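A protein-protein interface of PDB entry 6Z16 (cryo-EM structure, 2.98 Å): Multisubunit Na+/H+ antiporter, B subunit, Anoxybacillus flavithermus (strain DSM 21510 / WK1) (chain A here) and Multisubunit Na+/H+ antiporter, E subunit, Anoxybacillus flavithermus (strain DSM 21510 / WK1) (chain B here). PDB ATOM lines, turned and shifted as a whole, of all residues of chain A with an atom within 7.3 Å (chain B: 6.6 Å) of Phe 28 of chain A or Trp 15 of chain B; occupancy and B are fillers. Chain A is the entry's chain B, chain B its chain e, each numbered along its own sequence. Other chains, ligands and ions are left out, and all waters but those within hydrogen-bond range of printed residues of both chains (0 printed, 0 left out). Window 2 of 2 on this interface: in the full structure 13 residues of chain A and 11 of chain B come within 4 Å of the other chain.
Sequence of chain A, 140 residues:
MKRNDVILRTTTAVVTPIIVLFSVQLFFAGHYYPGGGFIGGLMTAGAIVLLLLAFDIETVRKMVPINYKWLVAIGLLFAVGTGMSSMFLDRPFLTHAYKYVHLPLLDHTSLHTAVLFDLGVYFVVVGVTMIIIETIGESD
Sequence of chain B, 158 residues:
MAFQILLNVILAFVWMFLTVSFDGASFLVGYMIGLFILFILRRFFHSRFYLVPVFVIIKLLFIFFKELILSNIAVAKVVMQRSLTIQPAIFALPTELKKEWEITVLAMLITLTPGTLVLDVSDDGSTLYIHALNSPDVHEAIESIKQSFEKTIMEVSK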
ATOM      1  N   VAL A  20     -15.671 -13.468 -25.574  1.00  0.00           N
ATOM      2  CA  VAL A  20     -15.176 -12.228 -26.167  1.00  0.00           C
ATOM      3  C   VAL A  20     -13.749 -12.399 -26.688  1.00  0.00           C
ATOM      4  O   VAL A  20     -13.432 -11.943 -27.797  1.00  0.00           O
ATOM      5  CB  VAL A  20     -15.297 -11.068 -25.163  1.00  0.00           C
ATOM      6  CG1 VAL A  20     -14.680  -9.809 -25.718  1.00  0.00           C
ATOM      7  CG2 VAL A  20     -16.750 -10.801 -24.857  1.00  0.00           C
ATOM      8  N   LEU A  21     -12.881 -13.084 -25.927  1.00  0.00           N
ATOM      9  CA  LEU A  21     -11.539 -13.397 -26.427  1.00  0.00           C
ATOM     10  C   LEU A  21     -11.587 -14.282 -27.661  1.00  0.00           C
ATOM     11  O   LEU A  21     -10.779 -14.110 -28.579  1.00  0.00           O
ATOM     12  CB  LEU A  21     -10.669 -14.084 -25.372  1.00  0.00           C
ATOM     13  CG  LEU A  21      -9.709 -13.339 -24.443  1.00  0.00           C
ATOM     14  CD1 LEU A  21     -10.359 -12.773 -23.227  1.00  0.00           C
ATOM     15  CD2 LEU A  21      -8.577 -14.249 -24.042  1.00  0.00           C
ATOM     16  N   PHE A  22     -12.531 -15.225 -27.709  1.00  0.00           N
ATOM     17  CA  PHE A  22     -12.639 -16.091 -28.874  1.00  0.00           C
ATOM     18  C   PHE A  22     -13.089 -15.318 -30.107  1.00  0.00           C
ATOM     19  O   PHE A  22     -12.572 -15.547 -31.204  1.00  0.00           O
ATOM     20  CB  PHE A  22     -13.583 -17.251 -28.567  1.00  0.00           C
ATOM     21  CG  PHE A  22     -13.771 -18.196 -29.710  1.00  0.00           C
ATOM     22  CD1 PHE A  22     -12.699 -18.919 -30.205  1.00  0.00           C
ATOM     23  CD2 PHE A  22     -15.025 -18.407 -30.252  1.00  0.00           C
ATOM     24  CE1 PHE A  22     -12.865 -19.801 -31.249  1.00  0.00           C
ATOM     25  CE2 PHE A  22     -15.199 -19.293 -31.292  1.00  0.00           C
ATOM     26  CZ  PHE A  22     -14.118 -19.992 -31.791  1.00  0.00           C
ATOM     27  N   SER A  23     -14.009 -14.366 -29.939  1.00  0.00           N
ATOM     28  CA  SER A  23     -14.470 -13.585 -31.082  1.00  0.00           C
ATOM     29  C   SER A  23     -13.389 -12.633 -31.583  1.00  0.00           C
ATOM     30  O   SER A  23     -13.212 -12.474 -32.797  1.00  0.00           O
ATOM     31  CB  SER A  23     -15.732 -12.816 -30.715  1.00  0.00           C
ATOM     32  OG  SER A  23     -15.450 -11.823 -29.753  1.00  0.00           O
ATOM     33  N   VAL A  24     -12.635 -12.017 -30.669  1.00  0.00           N
ATOM     34  CA  VAL A  24     -11.550 -11.126 -31.078  1.00  0.00           C
ATOM     35  C   VAL A  24     -10.420 -11.916 -31.733  1.00  0.00           C
ATOM     36  O   VAL A  24      -9.813 -11.462 -32.711  1.00  0.00           O
ATOM     37  CB  VAL A  24     -11.073 -10.301 -29.867  1.00  0.00           C
ATOM     38  CG1 VAL A  24      -9.836  -9.501 -30.176  1.00  0.00           C
ATOM     39  CG2 VAL A  24     -12.172  -9.356 -29.432  1.00  0.00           C
ATOM     40  N   GLN A  25     -10.154 -13.130 -31.246  1.00  0.00           N
ATOM     41  CA  GLN A  25      -9.143 -13.973 -31.874  1.00  0.00           C
ATOM     42  C   GLN A  25      -9.587 -14.470 -33.245  1.00  0.00           C
ATOM     43  O   GLN A  25      -8.755 -14.596 -34.152  1.00  0.00           O
ATOM     44  CB  GLN A  25      -8.808 -15.141 -30.948  1.00  0.00           C
ATOM     45  CG  GLN A  25      -7.746 -16.084 -31.477  1.00  0.00           C
ATOM     46  CD  GLN A  25      -6.424 -15.392 -31.711  1.00  0.00           C
ATOM     47  OE1 GLN A  25      -6.000 -14.554 -30.918  1.00  0.00           O
ATOM     48  NE2 GLN A  25      -5.763 -15.736 -32.808  1.00  0.00           N
ATOM     49  N   LEU A  26     -10.885 -14.747 -33.419  1.00  0.00           N
ATOM     50  CA  LEU A  26     -11.414 -15.044 -34.748  1.00  0.00           C
ATOM     51  C   LEU A  26     -11.262 -13.856 -35.684  1.00  0.00           C
ATOM     52  O   LEU A  26     -10.973 -14.026 -36.873  1.00  0.00           O
ATOM     53  CB  LEU A  26     -12.885 -15.445 -34.663  1.00  0.00           C
ATOM     54  CG  LEU A  26     -13.257 -16.834 -34.165  1.00  0.00           C
ATOM     55  CD1 LEU A  26     -14.757 -16.925 -34.000  1.00  0.00           C
ATOM     56  CD2 LEU A  26     -12.755 -17.866 -35.155  1.00  0.00           C
ATOM     57  N   PHE A  27     -11.442 -12.646 -35.161  1.00  0.00           N
ATOM     58  CA  PHE A  27     -11.359 -11.467 -36.012  1.00  0.00           C
ATOM     59  C   PHE A  27      -9.924 -11.144 -36.421  1.00  0.00           C
ATOM     60  O   PHE A  27      -9.671 -10.826 -37.586  1.00  0.00           O
ATOM     61  CB  PHE A  27     -12.002 -10.279 -35.315  1.00  0.00           C
ATOM     62  CG  PHE A  27     -11.826  -9.007 -36.052  1.00  0.00           C
ATOM     63  CD1 PHE A  27     -12.427  -8.822 -37.281  1.00  0.00           C
ATOM     64  CD2 PHE A  27     -11.069  -7.984 -35.515  1.00  0.00           C
ATOM     65  CE1 PHE A  27     -12.257  -7.650 -37.972  1.00  0.00           C
ATOM     66  CE2 PHE A  27     -10.899  -6.808 -36.199  1.00  0.00           C
ATOM     67  CZ  PHE A  27     -11.493  -6.642 -37.431  1.00  0.00           C
ATOM     68  N   PHE A  28      -8.972 -11.213 -35.486  1.00  0.00           N
ATOM     69  CA  PHE A  28      -7.602 -10.804 -35.801  1.00  0.00           C
ATOM     70  C   PHE A  28      -6.881 -11.810 -36.685  1.00  0.00           C
ATOM     71  O   PHE A  28      -5.997 -11.424 -37.455  1.00  0.00           O
ATOM     72  CB  PHE A  28      -6.793 -10.587 -34.522  1.00  0.00           C
ATOM     73  CG  PHE A  28      -7.111  -9.308 -33.804  1.00  0.00           C
ATOM     74  CD1 PHE A  28      -7.778  -8.283 -34.442  1.00  0.00           C
ATOM     75  CD2 PHE A  28      -6.724  -9.128 -32.488  1.00  0.00           C
ATOM     76  CE1 PHE A  28      -8.065  -7.110 -33.781  1.00  0.00           C
ATOM     77  CE2 PHE A  28      -7.005  -7.955 -31.823  1.00  0.00           C
ATOM     78  CZ  PHE A  28      -7.679  -6.946 -32.471  1.00  0.00           C
ATOM     79  N   ALA A  29      -7.228 -13.091 -36.595  1.00  0.00           N
ATOM     80  CA  ALA A  29      -6.556 -14.131 -37.364  1.00  0.00           C
ATOM     81  C   ALA A  29      -7.264 -14.443 -38.672  1.00  0.00           C
ATOM     82  O   ALA A  29      -7.157 -15.569 -39.172  1.00  0.00           O
ATOM     83  CB  ALA A  29      -6.422 -15.400 -36.525  1.00  0.00           C
ATOM     84  N   GLY A  30      -7.975 -13.473 -39.245  1.00  0.00           N
ATOM     85  CA  GLY A  30      -8.803 -13.759 -40.403  1.00  0.00           C
ATOM     86  C   GLY A  30      -8.012 -13.955 -41.681  1.00  0.00           C
ATOM     87  O   GLY A  30      -8.354 -14.807 -42.500  1.00  0.00           O
ATOM     88  N   HIS A  31      -6.951 -13.170 -41.875  1.00  0.00           N
ATOM     89  CA  HIS A  31      -6.201 -13.244 -43.124  1.00  0.00           C
ATOM     90  C   HIS A  31      -5.326 -14.478 -43.239  1.00  0.00           C
ATOM     91  O   HIS A  31      -4.921 -14.822 -44.352  1.00  0.00           O
ATOM     92  CB  HIS A  31      -5.308 -12.020 -43.308  1.00  0.00           C
ATOM     93  CG  HIS A  31      -6.017 -10.829 -43.860  1.00  0.00           C
ATOM     94  ND1 HIS A  31      -5.397  -9.611 -44.024  1.00  0.00           N
ATOM     95  CD2 HIS A  31      -7.285 -10.672 -44.303  1.00  0.00           C
ATOM     96  CE1 HIS A  31      -6.256  -8.751 -44.539  1.00  0.00           C
ATOM     97  NE2 HIS A  31      -7.409  -9.370 -44.719  1.00  0.00           N
ATOM     98  N   TYR A  32      -5.003 -15.137 -42.132  1.00  0.00           N
ATOM     99  CA  TYR A  32      -4.036 -16.224 -42.162  1.00  0.00           C
ATOM    100  C   TYR A  32      -4.635 -17.581 -41.852  1.00  0.00           C
ATOM    101  O   TYR A  32      -4.115 -18.594 -42.318  1.00  0.00           O
ATOM    102  CB  TYR A  32      -2.899 -15.939 -41.177  1.00  0.00           C
ATOM    103  CG  TYR A  32      -2.127 -14.693 -41.526  1.00  0.00           C
ATOM    104  CD1 TYR A  32      -1.102 -14.729 -42.457  1.00  0.00           C
ATOM    105  CD2 TYR A  32      -2.445 -13.470 -40.943  1.00  0.00           C
ATOM    106  CE1 TYR A  32      -0.402 -13.594 -42.788  1.00  0.00           C
ATOM    107  CE2 TYR A  32      -1.753 -12.328 -41.270  1.00  0.00           C
ATOM    108  CZ  TYR A  32      -0.733 -12.395 -42.193  1.00  0.00           C
ATOM    109  OH  TYR A  32      -0.042 -11.251 -42.514  1.00  0.00           O
ATOM    110  N   TYR A  33      -5.714 -17.621 -41.092  1.00  0.00           N
ATOM    111  CA  TYR A  33      -6.352 -18.851 -40.654  1.00  0.00           C
ATOM    112  C   TYR A  33      -7.847 -18.638 -40.864  1.00  0.00           C
ATOM    113  O   TYR A  33      -8.231 -17.516 -41.211  1.00  0.00           O
ATOM    114  CB  TYR A  33      -5.952 -19.135 -39.202  1.00  0.00           C
ATOM    115  CG  TYR A  33      -4.474 -19.377 -39.080  1.00  0.00           C
ATOM    116  CD1 TYR A  33      -3.909 -20.561 -39.532  1.00  0.00           C
ATOM    117  CD2 TYR A  33      -3.635 -18.412 -38.542  1.00  0.00           C
ATOM    118  CE1 TYR A  33      -2.554 -20.781 -39.446  1.00  0.00           C
ATOM    119  CE2 TYR A  33      -2.275 -18.623 -38.453  1.00  0.00           C
ATOM    120  CZ  TYR A  33      -1.743 -19.809 -38.904  1.00  0.00           C
ATOM    121  OH  TYR A  33      -0.391 -20.026 -38.810  1.00  0.00           O
ATOM    122  N   GLY A  35     -11.768 -17.794 -40.123  1.00  0.00           N
ATOM    123  CA  GLY A  35     -12.306 -16.708 -39.334  1.00  0.00           C
ATOM    124  C   GLY A  35     -12.364 -15.428 -40.145  1.00  0.00           C
ATOM    125  O   GLY A  35     -11.971 -15.376 -41.308  1.00  0.00           O
ATOM    126  N   GLY A  36     -12.864 -14.383 -39.501  1.00  0.00           N
ATOM    127  CA  GLY A  36     -12.944 -13.092 -40.156  1.00  0.00           C
ATOM    128  C   GLY A  36     -13.888 -12.171 -39.405  1.00  0.00           C
ATOM    129  O   GLY A  36     -14.214 -12.410 -38.247  1.00  0.00           O
ATOM    130  N   GLY A  37     -14.312 -11.115 -40.103  1.00  0.00           N
ATOM    131  CA  GLY A  37     -15.223 -10.157 -39.504  1.00  0.00           C
ATOM    132  C   GLY A  37     -16.613 -10.713 -39.275  1.00  0.00           C
ATOM    133  O   GLY A  37     -17.297 -10.306 -38.330  1.00  0.00           O
ATOM    134  N   VAL A 115      -7.757  -5.063 -43.342  1.00  0.00           N
ATOM    135  CA  VAL A 115      -8.174  -5.348 -41.978  1.00  0.00           C
ATOM    136  C   VAL A 115      -9.165  -4.300 -41.483  1.00  0.00           C
ATOM    137  O   VAL A 115     -10.087  -4.620 -40.729  1.00  0.00           O
ATOM    138  CB  VAL A 115      -6.922  -5.462 -41.091  1.00  0.00           C
ATOM    139  CG1 VAL A 115      -7.273  -5.803 -39.649  1.00  0.00           C
ATOM    140  CG2 VAL A 115      -5.978  -6.500 -41.673  1.00  0.00           C
ATOM    141  N   LEU A 119     -12.896  -4.639 -40.305  1.00  0.00           N
ATOM    142  CA  LEU A 119     -13.372  -4.014 -39.080  1.00  0.00           C
ATOM    143  C   LEU A 119     -14.724  -3.354 -39.301  1.00  0.00           C
ATOM    144  O   LEU A 119     -15.592  -3.381 -38.416  1.00  0.00           O
ATOM    145  CB  LEU A 119     -12.336  -3.012 -38.586  1.00  0.00           C
ATOM    146  CG  LEU A 119     -12.546  -2.377 -37.219  1.00  0.00           C
ATOM    147  CD1 LEU A 119     -12.560  -3.435 -36.149  1.00  0.00           C
ATOM    148  CD2 LEU A 119     -11.450  -1.387 -36.948  1.00  0.00           C
ATOM    149  N   ILE B  10      -4.352 -11.687 -15.501  1.00  0.00           N
ATOM    150  CA  ILE B  10      -4.488 -13.092 -15.875  1.00  0.00           C
ATOM    151  C   ILE B  10      -5.285 -13.240 -17.171  1.00  0.00           C
ATOM    152  O   ILE B  10      -5.068 -14.196 -17.920  1.00  0.00           O
ATOM    153  CB  ILE B  10      -5.065 -13.934 -14.713  1.00  0.00           C
ATOM    154  CG1 ILE B  10      -6.476 -13.514 -14.293  1.00  0.00           C
ATOM    155  CG2 ILE B  10      -4.131 -13.887 -13.513  1.00  0.00           C
ATOM    156  CD1 ILE B  10      -7.597 -14.367 -14.867  1.00  0.00           C
ATOM    157  N   LEU B  11      -6.179 -12.293 -17.493  1.00  0.00           N
ATOM    158  CA  LEU B  11      -6.802 -12.320 -18.816  1.00  0.00           C
ATOM    159  C   LEU B  11      -5.812 -11.979 -19.921  1.00  0.00           C
ATOM    160  O   LEU B  11      -5.924 -12.510 -21.029  1.00  0.00           O
ATOM    161  CB  LEU B  11      -7.999 -11.374 -18.895  1.00  0.00           C
ATOM    162  CG  LEU B  11      -9.293 -11.783 -18.200  1.00  0.00           C
ATOM    163  CD1 LEU B  11     -10.339 -10.711 -18.372  1.00  0.00           C
ATOM    164  CD2 LEU B  11      -9.798 -13.090 -18.757  1.00  0.00           C
ATOM    165  N   ALA B  12      -4.840 -11.107 -19.644  1.00  0.00           N
ATOM    166  CA  ALA B  12      -3.756 -10.907 -20.600  1.00  0.00           C
ATOM    167  C   ALA B  12      -2.910 -12.165 -20.760  1.00  0.00           C
ATOM    168  O   ALA B  12      -2.435 -12.457 -21.864  1.00  0.00           O
ATOM    169  CB  ALA B  12      -2.888  -9.733 -20.168  1.00  0.00           C
ATOM    170  N   PHE B  13      -2.735 -12.928 -19.676  1.00  0.00           N
ATOM    171  CA  PHE B  13      -2.064 -14.226 -19.772  1.00  0.00           C
ATOM    172  C   PHE B  13      -2.854 -15.208 -20.632  1.00  0.00           C
ATOM    173  O   PHE B  13      -2.272 -15.954 -21.427  1.00  0.00           O
ATOM    174  CB  PHE B  13      -1.845 -14.809 -18.375  1.00  0.00           C
ATOM    175  CG  PHE B  13      -0.747 -14.147 -17.599  1.00  0.00           C
ATOM    176  CD1 PHE B  13       0.247 -13.430 -18.243  1.00  0.00           C
ATOM    177  CD2 PHE B  13      -0.718 -14.234 -16.220  1.00  0.00           C
ATOM    178  CE1 PHE B  13       1.257 -12.824 -17.523  1.00  0.00           C
ATOM    179  CE2 PHE B  13       0.281 -13.629 -15.493  1.00  0.00           C
ATOM    180  CZ  PHE B  13       1.270 -12.921 -16.143  1.00  0.00           C
ATOM    181  N   VAL B  14      -4.184 -15.219 -20.480  1.00  0.00           N
ATOM    182  CA  VAL B  14      -5.037 -16.089 -21.291  1.00  0.00           C
ATOM    183  C   VAL B  14      -4.984 -15.674 -22.759  1.00  0.00           C
ATOM    184  O   VAL B  14      -4.977 -16.525 -23.655  1.00  0.00           O
ATOM    185  CB  VAL B  14      -6.476 -16.089 -20.733  1.00  0.00           C
ATOM    186  CG1 VAL B  14      -7.431 -16.854 -21.627  1.00  0.00           C
ATOM    187  CG2 VAL B  14      -6.501 -16.721 -19.366  1.00  0.00           C
ATOM    188  N   TRP B  15      -4.893 -14.367 -23.027  1.00  0.00           N
ATOM    189  CA  TRP B  15      -4.736 -13.907 -24.404  1.00  0.00           C
ATOM    190  C   TRP B  15      -3.390 -14.320 -24.990  1.00  0.00           C
ATOM    191  O   TRP B  15      -3.310 -14.679 -26.170  1.00  0.00           O
ATOM    192  CB  TRP B  15      -4.891 -12.390 -24.496  1.00  0.00           C
ATOM    193  CG  TRP B  15      -4.736 -11.919 -25.908  1.00  0.00           C
ATOM    194  CD1 TRP B  15      -3.622 -11.368 -26.477  1.00  0.00           C
ATOM    195  CD2 TRP B  15      -5.720 -11.986 -26.940  1.00  0.00           C
ATOM    196  NE1 TRP B  15      -3.856 -11.087 -27.799  1.00  0.00           N
ATOM    197  CE2 TRP B  15      -5.138 -11.456 -28.108  1.00  0.00           C
ATOM    198  CE3 TRP B  15      -7.038 -12.442 -26.991  1.00  0.00           C
ATOM    199  CZ2 TRP B  15      -5.829 -11.367 -29.309  1.00  0.00           C
ATOM    200  CZ3 TRP B  15      -7.720 -12.354 -28.181  1.00  0.00           C
ATOM    201  CH2 TRP B  15      -7.116 -11.820 -29.326  1.00  0.00           C
ATOM    202  N   MET B  16      -2.322 -14.261 -24.191  1.00  0.00           N
ATOM    203  CA  MET B  16      -1.020 -14.702 -24.683  1.00  0.00           C
ATOM    204  C   MET B  16      -0.980 -16.209 -24.894  1.00  0.00           C
ATOM    205  O   MET B  16      -0.243 -16.698 -25.758  1.00  0.00           O
ATOM    206  CB  MET B  16       0.087 -14.287 -23.718  1.00  0.00           C
ATOM    207  CG  MET B  16       0.322 -12.798 -23.625  1.00  0.00           C
ATOM    208  SD  MET B  16       1.579 -12.406 -22.397  1.00  0.00           S
ATOM    209  CE  MET B  16       3.051 -12.969 -23.240  1.00  0.00           C
ATOM    210  N   PHE B  17      -1.762 -16.955 -24.116  1.00  0.00           N
ATOM    211  CA  PHE B  17      -1.836 -18.402 -24.252  1.00  0.00           C
ATOM    212  C   PHE B  17      -2.751 -18.836 -25.388  1.00  0.00           C
ATOM    213  O   PHE B  17      -2.570 -19.931 -25.929  1.00  0.00           O
ATOM    214  CB  PHE B  17      -2.311 -19.007 -22.931  1.00  0.00           C
ATOM    215  CG  PHE B  17      -2.370 -20.499 -22.929  1.00  0.00           C
ATOM    216  CD1 PHE B  17      -1.208 -21.247 -22.877  1.00  0.00           C
ATOM    217  CD2 PHE B  17      -3.589 -21.156 -22.967  1.00  0.00           C
ATOM    218  CE1 PHE B  17      -1.257 -22.621 -22.871  1.00  0.00           C
ATOM    219  CE2 PHE B  17      -3.646 -22.531 -22.962  1.00  0.00           C
ATOM    220  CZ  PHE B  17      -2.476 -23.266 -22.916  1.00  0.00           C
ATOM    221  N   LEU B  18      -3.717 -17.997 -25.763  1.00  0.00           N
ATOM    222  CA  LEU B  18      -4.653 -18.346 -26.825  1.00  0.00           C
ATOM    223  C   LEU B  18      -3.969 -18.344 -28.184  1.00  0.00           C
ATOM    224  O   LEU B  18      -4.378 -19.086 -29.082  1.00  0.00           O
ATOM    225  CB  LEU B  18      -5.832 -17.377 -26.801  1.00  0.00           C
ATOM    226  CG  LEU B  18      -7.053 -17.677 -27.661  1.00  0.00           C
ATOM    227  CD1 LEU B  18      -7.676 -18.974 -27.206  1.00  0.00           C
ATOM    228  CD2 LEU B  18      -8.049 -16.550 -27.546  1.00  0.00           C
ATOM    229  N   THR B  19      -2.934 -17.530 -28.350  1.00  0.00           N
ATOM    230  CA  THR B  19      -1.987 -17.671 -29.443  1.00  0.00           C
ATOM    231  C   THR B  19      -0.738 -18.378 -28.926  1.00  0.00           C
ATOM    232  O   THR B  19      -0.665 -18.806 -27.774  1.00  0.00           O
ATOM    233  CB  THR B  19      -1.633 -16.312 -30.046  1.00  0.00           C
ATOM    234  OG1 THR B  19      -1.002 -15.497 -29.053  1.00  0.00           O
ATOM    235  CG2 THR B  19      -2.878 -15.615 -30.541  1.00  0.00           C
ATOM    236  N   VAL B  20       0.267 -18.498 -29.788  1.00  0.00           N
ATOM    237  CA  VAL B  20       1.477 -19.234 -29.452  1.00  0.00           C
ATOM    238  C   VAL B  20       2.694 -18.324 -29.373  1.00  0.00           C
ATOM    239  O   VAL B  20       3.825 -18.814 -29.298  1.00  0.00           O
ATOM    240  CB  VAL B  20       1.715 -20.388 -30.440  1.00  0.00           C
ATOM    241  CG1 VAL B  20       0.565 -21.386 -30.367  1.00  0.00           C
ATOM    242  CG2 VAL B  20       1.878 -19.852 -31.853  1.00  0.00           C
ATOM    243  N   SER B  21       2.494 -17.011 -29.380  1.00  0.00           N
ATOM    244  CA  SER B  21       3.582 -16.052 -29.260  1.00  0.00           C
ATOM    245  C   SER B  21       3.596 -15.462 -27.858  1.00  0.00           C
ATOM    246  O   SER B  21       2.548 -15.100 -27.315  1.00  0.00           O
ATOM    247  CB  SER B  21       3.444 -14.932 -30.291  1.00  0.00           C
ATOM    248  OG  SER B  21       2.300 -14.140 -30.033  1.00  0.00           O
ATOM    249  N   SER B  26       2.110  -8.557 -27.286  1.00  0.00           N
ATOM    250  CA  SER B  26       0.889  -9.336 -27.124  1.00  0.00           C
ATOM    251  C   SER B  26       0.320  -9.198 -25.720  1.00  0.00           C
ATOM    252  O   SER B  26      -0.899  -9.278 -25.542  1.00  0.00           O
ATOM    253  CB  SER B  26       1.162 -10.802 -27.449  1.00  0.00           C
ATOM    254  OG  SER B  26       2.059 -11.363 -26.512  1.00  0.00           O
ATOM    255  N   PHE B  27       1.179  -8.960 -24.723  1.00  0.00           N
ATOM    256  CA  PHE B  27       0.696  -8.716 -23.369  1.00  0.00           C
ATOM    257  C   PHE B  27      -0.065  -7.400 -23.281  1.00  0.00           C
ATOM    258  O   PHE B  27      -1.107  -7.327 -22.623  1.00  0.00           O
ATOM    259  CB  PHE B  27       1.862  -8.726 -22.380  1.00  0.00           C
ATOM    260  CG  PHE B  27       1.445  -8.523 -20.952  1.00  0.00           C
ATOM    261  CD1 PHE B  27       0.869  -9.555 -20.233  1.00  0.00           C
ATOM    262  CD2 PHE B  27       1.624  -7.299 -20.333  1.00  0.00           C
ATOM    263  CE1 PHE B  27       0.481  -9.371 -18.920  1.00  0.00           C
ATOM    264  CE2 PHE B  27       1.235  -7.108 -19.023  1.00  0.00           C
ATOM    265  CZ  PHE B  27       0.662  -8.146 -18.316  1.00  0.00           C
ATOM    266  N   VAL B  29      -1.599  -5.954 -25.844  1.00  0.00           N
ATOM    267  CA  VAL B  29      -2.829  -6.174 -26.611  1.00  0.00           C
ATOM    268  C   VAL B  29      -3.871  -6.897 -25.760  1.00  0.00           C
ATOM    269  O   VAL B  29      -5.033  -6.472 -25.671  1.00  0.00           O
ATOM    270  CB  VAL B  29      -2.528  -6.947 -27.907  1.00  0.00           C
ATOM    271  CG1 VAL B  29      -3.814  -7.306 -28.619  1.00  0.00           C
ATOM    272  CG2 VAL B  29      -1.664  -6.121 -28.827  1.00  0.00           C
ATOM    273  N   GLY B  30      -3.455  -7.973 -25.087  1.00  0.00           N
ATOM    274  CA  GLY B  30      -4.355  -8.692 -24.206  1.00  0.00           C
ATOM    275  C   GLY B  30      -4.788  -7.890 -23.000  1.00  0.00           C
ATOM    276  O   GLY B  30      -5.906  -8.063 -22.512  1.00  0.00           O
ATOM    277  N   TYR B  31      -3.938  -6.974 -22.531  1.00  0.00           N
ATOM    278  CA  TYR B  31      -4.316  -6.127 -21.406  1.00  0.00           C
ATOM    279  C   TYR B  31      -5.367  -5.104 -21.817  1.00  0.00           C
ATOM    280  O   TYR B  31      -6.279  -4.805 -21.041  1.00  0.00           O
ATOM    281  CB  TYR B  31      -3.081  -5.433 -20.831  1.00  0.00           C
ATOM    282  CG  TYR B  31      -3.380  -4.625 -19.591  1.00  0.00           C
ATOM    283  CD1 TYR B  31      -3.545  -5.246 -18.362  1.00  0.00           C
ATOM    284  CD2 TYR B  31      -3.522  -3.243 -19.653  1.00  0.00           C
ATOM    285  CE1 TYR B  31      -3.828  -4.514 -17.226  1.00  0.00           C
ATOM    286  CE2 TYR B  31      -3.812  -2.503 -18.524  1.00  0.00           C
ATOM    287  CZ  TYR B  31      -3.962  -3.146 -17.315  1.00  0.00           C
ATOM    288  OH  TYR B  31      -4.247  -2.415 -16.187  1.00  0.00           O
ATOM    289  N   ILE B  33      -7.567  -5.586 -24.322  1.00  0.00           N
ATOM    290  CA  ILE B  33      -8.772  -6.400 -24.503  1.00  0.00           C
ATOM    291  C   ILE B  33      -9.415  -6.720 -23.157  1.00  0.00           C
ATOM    292  O   ILE B  33     -10.636  -6.596 -22.991  1.00  0.00           O
ATOM    293  CB  ILE B  33      -8.432  -7.677 -25.295  1.00  0.00           C
ATOM    294  CG1 ILE B  33      -7.997  -7.330 -26.712  1.00  0.00           C
ATOM    295  CG2 ILE B  33      -9.616  -8.604 -25.380  1.00  0.00           C
ATOM    296  CD1 ILE B  33      -7.387  -8.485 -27.440  1.00  0.00           C
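Among the printed residues, pairs that only touch across the chains: Leu 21 of chain A with Val 14 of chain B, Leu 21 of chain A with Trp 15 of chain B, Leu 21 of chain A with Leu 18 of chain B, Val 24 of chain A with Trp 15 of chain B, Val 24 of chain A with Ile 33 of chain B, Gln 25 of chain A with Trp 15 of chain B, Gln 25 of chain A with Leu 18 of chain B, Gln 25 of chain A with Thr 19 of chain B and Phe 28 of chain A with Trp 15 of chain B.
Of the printed residues of chain B, Leu 21 of chain A touches Val 14, Trp 15 and Leu 18. Of the printed residues of chain B, Gln 25 of chain A touches Trp 15 (3.4 Å), Leu 18 (3.8 Å) and Thr 19 (3.3 Å). Printed residues of chain B within 4 Å of Phe 28 of chain A: Trp 15 (3.99 Å). Of the printed residues of chain A, Val 14 of chain B touches Leu 21. Printed residues of chain A within 4 Å of Trp 15 of chain B: Leu 21, Val 24, Gln 25 and Phe 28. Printed residues of chain A within 4 Å of Leu 18 of chain B: Leu 21 (3.8 Å) and Gln 25 (3.8 Å). Of the printed residues of chain A, Ile 33 of chain B touches Val 24. The nearest printed residue of chain B that does not touch Phe 28 of chain A is Ile 33 of chain B (4.4 Å). The nearest printed residue of chain A that does not touch Trp 15 of chain B is Phe 22 of chain A (5.6 Å).
Printed residues of chain B that touch a printed residue of chain A: Val 14, Trp 15, Leu 18, Thr 19 and Ile 33. Hydrophobic or aromatic side chains of chain B within 4 Å of the printed part of chain A: Val 14, Trp 15, Leu 18 and Ile 33. Of the 19 printed residues of chain A, 4 touch a printed residue of chain B. Printed residues of chain A that touch a printed residue of chain B: Leu 21, Val 24, Gln 25 and Phe 28. Hydrophobic or aromatic side chains of chain A that line the printed part of chain B: Leu 21, Val 24 and Phe 28. Among the printed residues, 9 pairs touch across the chains. Among the printed residues, no Asp or Glu carboxylate lies within 4 Å of a Lys or Arg side-chain nitrogen of the other chain.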
